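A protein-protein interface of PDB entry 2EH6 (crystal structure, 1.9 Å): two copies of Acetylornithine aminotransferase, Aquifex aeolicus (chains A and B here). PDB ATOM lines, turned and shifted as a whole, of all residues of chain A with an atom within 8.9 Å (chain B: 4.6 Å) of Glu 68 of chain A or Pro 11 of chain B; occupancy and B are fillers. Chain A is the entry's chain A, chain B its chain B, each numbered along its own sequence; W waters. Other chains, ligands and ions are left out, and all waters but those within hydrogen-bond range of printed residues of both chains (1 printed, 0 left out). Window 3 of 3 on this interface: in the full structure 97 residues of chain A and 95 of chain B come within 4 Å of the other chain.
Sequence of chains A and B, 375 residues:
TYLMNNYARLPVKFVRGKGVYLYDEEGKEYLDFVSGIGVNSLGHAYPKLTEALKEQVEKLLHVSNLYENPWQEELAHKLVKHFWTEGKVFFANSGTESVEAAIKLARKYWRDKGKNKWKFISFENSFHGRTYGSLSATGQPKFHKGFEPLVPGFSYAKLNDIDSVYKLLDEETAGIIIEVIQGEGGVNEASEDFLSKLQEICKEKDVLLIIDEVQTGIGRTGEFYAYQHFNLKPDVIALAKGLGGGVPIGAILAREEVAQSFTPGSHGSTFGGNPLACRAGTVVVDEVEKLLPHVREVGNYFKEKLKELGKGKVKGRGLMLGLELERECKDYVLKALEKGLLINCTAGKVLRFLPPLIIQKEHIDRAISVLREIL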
ATOM      1  N   LEU A  60     -15.624  15.775 -17.349  1.00  0.00           N
ATOM      2  CA  LEU A  60     -15.430  16.224 -18.719  1.00  0.00           C
ATOM      3  C   LEU A  60     -16.752  16.366 -19.463  1.00  0.00           C
ATOM      4  O   LEU A  60     -17.571  15.449 -19.468  1.00  0.00           O
ATOM      5  CB  LEU A  60     -14.549  15.194 -19.433  1.00  0.00           C
ATOM      6  CG  LEU A  60     -13.874  15.522 -20.751  1.00  0.00           C
ATOM      7  CD1 LEU A  60     -12.944  16.709 -20.553  1.00  0.00           C
ATOM      8  CD2 LEU A  60     -13.089  14.293 -21.231  1.00  0.00           C
ATOM      9  N   VAL A  63     -14.594  17.284 -25.535  1.00  0.00           N
ATOM     10  CA  VAL A  63     -13.215  17.459 -26.015  1.00  0.00           C
ATOM     11  C   VAL A  63     -13.124  17.632 -27.549  1.00  0.00           C
ATOM     12  O   VAL A  63     -12.119  18.067 -28.092  1.00  0.00           O
ATOM     13  CB  VAL A  63     -12.404  16.229 -25.583  1.00  0.00           C
ATOM     14  CG1 VAL A  63     -12.446  16.072 -24.062  1.00  0.00           C
ATOM     15  CG2 VAL A  63     -12.973  14.988 -26.238  1.00  0.00           C
ATOM     16  N   SER A  64     -14.227  17.245 -28.241  1.00  0.00           N
ATOM     17  CA  SER A  64     -14.288  17.205 -29.722  1.00  0.00           C
ATOM     18  C   SER A  64     -13.722  15.916 -30.312  1.00  0.00           C
ATOM     19  O   SER A  64     -12.949  15.191 -29.706  1.00  0.00           O
ATOM     20  CB  SER A  64     -13.593  18.403 -30.368  1.00  0.00           C
ATOM     21  OG  SER A  64     -12.224  18.088 -30.598  1.00  0.00           O
ATOM     22  N   ASN A  65     -14.151  15.651 -31.565  1.00  0.00           N
ATOM     23  CA  ASN A  65     -13.662  14.473 -32.273  1.00  0.00           C
ATOM     24  C   ASN A  65     -12.280  14.688 -32.909  1.00  0.00           C
ATOM     25  O   ASN A  65     -11.878  13.973 -33.821  1.00  0.00           O
ATOM     26  CB  ASN A  65     -14.687  14.096 -33.342  1.00  0.00           C
ATOM     27  CG  ASN A  65     -15.958  13.631 -32.674  1.00  0.00           C
ATOM     28  OD1 ASN A  65     -15.986  12.645 -31.942  1.00  0.00           O
ATOM     29  ND2 ASN A  65     -17.042  14.378 -32.941  1.00  0.00           N
ATOM     30  N   LEU A  66     -11.564  15.738 -32.438  1.00  0.00           N
ATOM     31  CA  LEU A  66     -10.152  15.868 -32.810  1.00  0.00           C
ATOM     32  C   LEU A  66      -9.334  14.750 -32.158  1.00  0.00           C
ATOM     33  O   LEU A  66      -8.272  14.352 -32.618  1.00  0.00           O
ATOM     34  CB  LEU A  66      -9.624  17.216 -32.303  1.00  0.00           C
ATOM     35  CG  LEU A  66     -10.222  18.428 -33.020  1.00  0.00           C
ATOM     36  CD1 LEU A  66      -9.731  19.752 -32.425  1.00  0.00           C
ATOM     37  CD2 LEU A  66      -9.872  18.468 -34.504  1.00  0.00           C
ATOM     38  N   TYR A  67      -9.855  14.284 -31.003  1.00  0.00           N
ATOM     39  CA  TYR A  67      -9.176  13.251 -30.234  1.00  0.00           C
ATOM     40  C   TYR A  67     -10.015  11.969 -30.159  1.00  0.00           C
ATOM     41  O   TYR A  67     -11.142  11.903 -30.632  1.00  0.00           O
ATOM     42  CB  TYR A  67      -8.892  13.789 -28.820  1.00  0.00           C
ATOM     43  CG  TYR A  67      -8.479  15.223 -28.866  1.00  0.00           C
ATOM     44  CD1 TYR A  67      -7.177  15.562 -29.221  1.00  0.00           C
ATOM     45  CD2 TYR A  67      -9.388  16.229 -28.533  1.00  0.00           C
ATOM     46  CE1 TYR A  67      -6.785  16.892 -29.245  1.00  0.00           C
ATOM     47  CE2 TYR A  67      -8.994  17.558 -28.549  1.00  0.00           C
ATOM     48  CZ  TYR A  67      -7.697  17.890 -28.895  1.00  0.00           C
ATOM     49  OH  TYR A  67      -7.293  19.210 -28.898  1.00  0.00           O
ATOM     50  N   GLU A  68      -9.446  10.957 -29.509  1.00  0.00           N
ATOM     51  CA  GLU A  68     -10.142   9.697 -29.285  1.00  0.00           C
ATOM     52  C   GLU A  68     -11.234   9.901 -28.240  1.00  0.00           C
ATOM     53  O   GLU A  68     -10.998  10.524 -27.209  1.00  0.00           O
ATOM     54  CB  GLU A  68      -9.177   8.631 -28.767  1.00  0.00           C
ATOM     55  CG  GLU A  68      -8.252   8.039 -29.804  1.00  0.00           C
ATOM     56  CD  GLU A  68      -7.286   7.046 -29.188  1.00  0.00           C
ATOM     57  OE1 GLU A  68      -7.745   6.191 -28.397  1.00  0.00           O
ATOM     58  OE2 GLU A  68      -6.077   7.113 -29.492  1.00  0.00           O
ATOM     59  N   ASN A  69     -12.424   9.375 -28.514  1.00  0.00           N
ATOM     60  CA  ASN A  69     -13.554   9.470 -27.590  1.00  0.00           C
ATOM     61  C   ASN A  69     -13.977   8.046 -27.225  1.00  0.00           C
ATOM     62  O   ASN A  69     -14.933   7.510 -27.790  1.00  0.00           O
ATOM     63  CB  ASN A  69     -14.736  10.204 -28.245  1.00  0.00           C
ATOM     64  CG  ASN A  69     -14.523  11.706 -28.337  1.00  0.00           C
ATOM     65  OD1 ASN A  69     -15.355  12.481 -27.872  1.00  0.00           O
ATOM     66  ND2 ASN A  69     -13.416  12.122 -28.950  1.00  0.00           N
ATOM     67  N   PRO A  70     -13.269   7.415 -26.273  1.00  0.00           N
ATOM     68  CA  PRO A  70     -13.562   6.045 -25.832  1.00  0.00           C
ATOM     69  C   PRO A  70     -15.023   5.805 -25.460  1.00  0.00           C
ATOM     70  O   PRO A  70     -15.554   4.710 -25.653  1.00  0.00           O
ATOM     71  CB  PRO A  70     -12.622   5.861 -24.641  1.00  0.00           C
ATOM     72  CG  PRO A  70     -11.448   6.733 -25.006  1.00  0.00           C
ATOM     73  CD  PRO A  70     -12.137   7.976 -25.513  1.00  0.00           C
ATOM     74  N   TRP A  71     -15.670   6.824 -24.908  1.00  0.00           N
ATOM     75  CA  TRP A  71     -17.075   6.704 -24.527  1.00  0.00           C
ATOM     76  C   TRP A  71     -17.941   6.463 -25.762  1.00  0.00           C
ATOM     77  O   TRP A  71     -18.995   5.835 -25.671  1.00  0.00           O
ATOM     78  CB  TRP A  71     -17.521   7.961 -23.781  1.00  0.00           C
ATOM     79  CG  TRP A  71     -16.985   9.216 -24.373  1.00  0.00           C
ATOM     80  CD1 TRP A  71     -17.505   9.918 -25.421  1.00  0.00           C
ATOM     81  CD2 TRP A  71     -15.797   9.909 -23.973  1.00  0.00           C
ATOM     82  NE1 TRP A  71     -16.715  11.006 -25.698  1.00  0.00           N
ATOM     83  CE2 TRP A  71     -15.659  11.024 -24.825  1.00  0.00           C
ATOM     84  CE3 TRP A  71     -14.835   9.695 -22.973  1.00  0.00           C
ATOM     85  CZ2 TRP A  71     -14.595  11.926 -24.714  1.00  0.00           C
ATOM     86  CZ3 TRP A  71     -13.775  10.594 -22.861  1.00  0.00           C
ATOM     87  CH2 TRP A  71     -13.665  11.696 -23.730  1.00  0.00           C
ATOM     88  N   GLN A  72     -17.504   6.968 -26.913  1.00  0.00           N
ATOM     89  CA  GLN A  72     -18.243   6.748 -28.159  1.00  0.00           C
ATOM     90  C   GLN A  72     -18.149   5.260 -28.520  1.00  0.00           C
ATOM     91  O   GLN A  72     -19.137   4.643 -28.921  1.00  0.00           O
ATOM     92  CB  GLN A  72     -17.661   7.604 -29.298  1.00  0.00           C
ATOM     93  CG  GLN A  72     -18.234   9.026 -29.366  1.00  0.00           C
ATOM     94  CD  GLN A  72     -17.573   9.893 -30.436  1.00  0.00           C
ATOM     95  OE1 GLN A  72     -17.380   9.465 -31.576  1.00  0.00           O
ATOM     96  NE2 GLN A  72     -17.237  11.121 -30.071  1.00  0.00           N
ATOM     97  N   GLU A  73     -16.957   4.688 -28.372  1.00  0.00           N
ATOM     98  CA  GLU A  73     -16.758   3.268 -28.668  1.00  0.00           C
ATOM     99  C   GLU A  73     -17.683   2.402 -27.821  1.00  0.00           C
ATOM    100  O   GLU A  73     -18.356   1.516 -28.340  1.00  0.00           O
ATOM    101  CB  GLU A  73     -15.312   2.845 -28.383  1.00  0.00           C
ATOM    102  CG  GLU A  73     -14.292   3.300 -29.398  1.00  0.00           C
ATOM    103  CD  GLU A  73     -14.481   2.656 -30.759  1.00  0.00           C
ATOM    104  OE1 GLU A  73     -15.150   1.601 -30.846  1.00  0.00           O
ATOM    105  OE2 GLU A  73     -13.942   3.203 -31.742  1.00  0.00           O
ATOM    106  N   GLY A 273     -21.141  13.005 -30.068  1.00  0.00           N
ATOM    107  CA  GLY A 273     -20.387  12.027 -29.297  1.00  0.00           C
ATOM    108  C   GLY A 273     -19.617  12.543 -28.096  1.00  0.00           C
ATOM    109  O   GLY A 273     -18.644  11.925 -27.659  1.00  0.00           O
ATOM    110  N   PRO A 275     -18.727  13.291 -24.212  1.00  0.00           N
ATOM    111  CA  PRO A 275     -18.865  12.376 -23.070  1.00  0.00           C
ATOM    112  C   PRO A 275     -20.148  12.468 -22.239  1.00  0.00           C
ATOM    113  O   PRO A 275     -20.547  11.489 -21.614  1.00  0.00           O
ATOM    114  CB  PRO A 275     -17.601  12.652 -22.247  1.00  0.00           C
ATOM    115  CG  PRO A 275     -17.272  14.080 -22.588  1.00  0.00           C
ATOM    116  CD  PRO A 275     -17.525  14.131 -24.074  1.00  0.00           C
ATOM    117  N   ARG B   9      -8.750  11.333 -35.950  1.00  0.00           N
ATOM    118  CA  ARG B   9      -8.446  11.546 -34.540  1.00  0.00           C
ATOM    119  C   ARG B   9      -6.976  11.470 -34.123  1.00  0.00           C
ATOM    120  O   ARG B   9      -6.234  10.599 -34.578  1.00  0.00           O
ATOM    121  CB  ARG B   9      -9.228  10.539 -33.701  1.00  0.00           C
ATOM    122  CG  ARG B   9     -10.716  10.472 -33.991  1.00  0.00           C
ATOM    123  CD  ARG B   9     -11.353   9.448 -33.072  1.00  0.00           C
ATOM    124  NE  ARG B   9     -12.759   9.193 -33.356  1.00  0.00           N
ATOM    125  CZ  ARG B   9     -13.771   9.939 -32.921  1.00  0.00           C
ATOM    126  NH1 ARG B   9     -13.549  11.012 -32.171  1.00  0.00           N
ATOM    127  NH2 ARG B   9     -15.013   9.592 -33.221  1.00  0.00           N
ATOM    128  N   LEU B  10      -6.562  12.382 -33.247  1.00  0.00           N
ATOM    129  CA  LEU B  10      -5.197  12.367 -32.732  1.00  0.00           C
ATOM    130  C   LEU B  10      -5.104  11.185 -31.768  1.00  0.00           C
ATOM    131  O   LEU B  10      -6.065  10.873 -31.058  1.00  0.00           O
ATOM    132  CB  LEU B  10      -4.876  13.663 -31.987  1.00  0.00           C
ATOM    133  CG  LEU B  10      -4.579  14.889 -32.849  1.00  0.00           C
ATOM    134  CD1 LEU B  10      -4.348  16.102 -31.962  1.00  0.00           C
ATOM    135  CD2 LEU B  10      -3.351  14.608 -33.710  1.00  0.00           C
ATOM    136  N   PRO B  11      -3.941  10.514 -31.726  1.00  0.00           N
ATOM    137  CA  PRO B  11      -3.715   9.357 -30.853  1.00  0.00           C
ATOM    138  C   PRO B  11      -3.630   9.681 -29.360  1.00  0.00           C
ATOM    139  O   PRO B  11      -2.625   9.392 -28.709  1.00  0.00           O
ATOM    140  CB  PRO B  11      -2.412   8.779 -31.393  1.00  0.00           C
ATOM    141  CG  PRO B  11      -1.663  10.011 -31.778  1.00  0.00           C
ATOM    142  CD  PRO B  11      -2.725  10.825 -32.500  1.00  0.00           C
ATOM    143  N   VAL B  12      -4.691  10.274 -28.822  1.00  0.00           N
ATOM    144  CA  VAL B  12      -4.728  10.620 -27.408  1.00  0.00           C
ATOM    145  C   VAL B  12      -6.162  10.604 -26.897  1.00  0.00           C
ATOM    146  O   VAL B  12      -7.094  10.970 -27.617  1.00  0.00           O
ATOM    147  CB  VAL B  12      -4.114  12.016 -27.157  1.00  0.00           C
ATOM    148  CG1 VAL B  12      -4.977  13.092 -27.806  1.00  0.00           C
ATOM    149  CG2 VAL B  12      -3.958  12.261 -25.662  1.00  0.00           C
ATOM    150  N   LYS B  13      -6.339  10.153 -25.661  1.00  0.00           N
ATOM    151  CA  LYS B  13      -7.659  10.110 -25.063  1.00  0.00           C
ATOM    152  C   LYS B  13      -7.628  10.695 -23.656  1.00  0.00           C
ATOM    153  O   LYS B  13      -6.855  10.265 -22.797  1.00  0.00           O
ATOM    154  CB  LYS B  13      -8.203   8.677 -25.057  1.00  0.00           C
ATOM    155  CG  LYS B  13      -7.439   7.691 -24.206  1.00  0.00           C
ATOM    156  CD  LYS B  13      -7.940   6.275 -24.473  1.00  0.00           C
ATOM    157  CE  LYS B  13      -7.450   5.295 -23.418  1.00  0.00           C
ATOM    158  NZ  LYS B  13      -8.135   5.516 -22.109  1.00  0.00           N
ATOM    159  N   LEU B 334       1.561  17.170 -33.699  1.00  0.00           N
ATOM    160  CA  LEU B 334       2.017  15.982 -32.988  1.00  0.00           C
ATOM    161  C   LEU B 334       3.167  16.311 -32.048  1.00  0.00           C
ATOM    162  O   LEU B 334       3.202  15.846 -30.909  1.00  0.00           O
ATOM    163  CB  LEU B 334       2.447  14.901 -33.983  1.00  0.00           C
ATOM    164  CG  LEU B 334       1.304  14.250 -34.765  1.00  0.00           C
ATOM    165  CD1 LEU B 334       1.864  13.338 -35.855  1.00  0.00           C
ATOM    166  CD2 LEU B 334       0.419  13.466 -33.796  1.00  0.00           C
HETATM  167  O   HOH W   1     -13.010   7.679 -30.388  1.00  0.00           O
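Of the 6 printed residues of chain B, 5 touch a printed residue of chain A. Printed residues of chain B that touch a printed residue of chain A: Arg 9, Leu 10, Pro 11, Val 12 and Lys 13. Among the printed residues, no Asp or Glu carboxylate lies within 4 Å of a Lys or Arg side-chain nitrogen of the other chain.
NH1 of Arg 9 of chain B sits at hydrogen-bond distance from OD1 of Asn 65 of chain A (2.9 Å). O of Leu 66 of chain A is in hydrogen-bond range of N of Leu 10 of chain B (2.7 Å). The guanidinium group of Arg 9 of chain B is in hydrogen-bond range of the backbone carbonyl oxygen of Tyr 67 of chain A (3.0 Å). N of Glu 68 of chain A sits at hydrogen-bond distance from O of Val 12 of chain B (3.0 Å). The guanidinium group of Arg 9 of chain B lies close to the side-chain amide nitrogen of Asn 69 of chain A. The side-chain amide oxygen (OE1) of Gln 72 of chain A sits at hydrogen-bond distance from the guanidinium group (NH2) of Arg 9 of chain B, at 2.9 Å.
No position is printed for both chains.
OG of Ser 64 of chain A sits close to N of Leu 66 of chain A, at 3.1 Å. The side-chain amide nitrogen of Gln 72 of chain A sits at hydrogen-bond distance from the side-chain amide oxygen of Asn 65 of chain A, at 2.7 Å. The side-chain amide nitrogen of Asn 69 of chain A is in hydrogen-bond range of the backbone carbonyl oxygen of Tyr 67 of chain A (2.8 Å). NE1 of Trp 71 of chain A lies within hydrogen-bond range of OD1 of Asn 69 of chain A, 3.0 Å away. The side-chain amide oxygen (OD1) of Asn 69 of chain A lies within hydrogen-bond range of the side-chain amide nitrogen (NE2) of Gln 72 of chain A, 3.2 Å away. The side-chain amide oxygen (OD1) of Asn 69 of chain A lies close to the backbone carbonyl oxygen (O) of Gly 273 of chain A.
Arg 9 of chain B touches Leu 66 of chain A (CA to O, 3.4 Å). Tyr 67 of chain A touches Leu 10 of chain B. Val 12 of chain B touches Tyr 67 of chain A (O to CB, 3.6 Å). Glu 68 of chain A touches Arg 9 of chain B (CA to CD, 3.98 Å). Leu 10 of chain B touches Glu 68 of chain A. Glu 68 of chain A touches Pro 11 of chain B. Lys 13 of chain B touches Glu 68 of chain A. CD of Lys 13 of chain B touches CG of Pro 70 of chain A (3.6 Å).
Water W1 bridges the backbone NH of Asn 69 of chain A and the guanidinium group of Arg 9 of chain B.
Val 63 of chain A touches none of the printed residues of chain B. Of the printed residues of chain B, Glu 68 of chain A touches Arg 9 (3.98 Å), Leu 10 (3.7 Å), Pro 11 (3.5 Å), Val 12 (3.0 Å) and Lys 13 (3.8 Å). Of the printed residues of chain B, Asn 69 of chain A touches Arg 9. Pro 275 of chain A touches none of the printed residues of chain B. Of the printed residues of chain A, Arg 9 of chain B touches Asn 65 (2.9 Å), Leu 66 (3.4 Å), Tyr 67 (3.0 Å), Glu 68 (3.98 Å), Asn 69 (3.4 Å) and Gln 72 (2.9 Å). Of chain A, only Glu 68 (3.5 Å) comes within 4 Å of Pro 11 of chain B. Val 12 of chain B touches just these residues of chain A: Tyr 67 (3.6 Å) and Glu 68 (3.0 Å).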
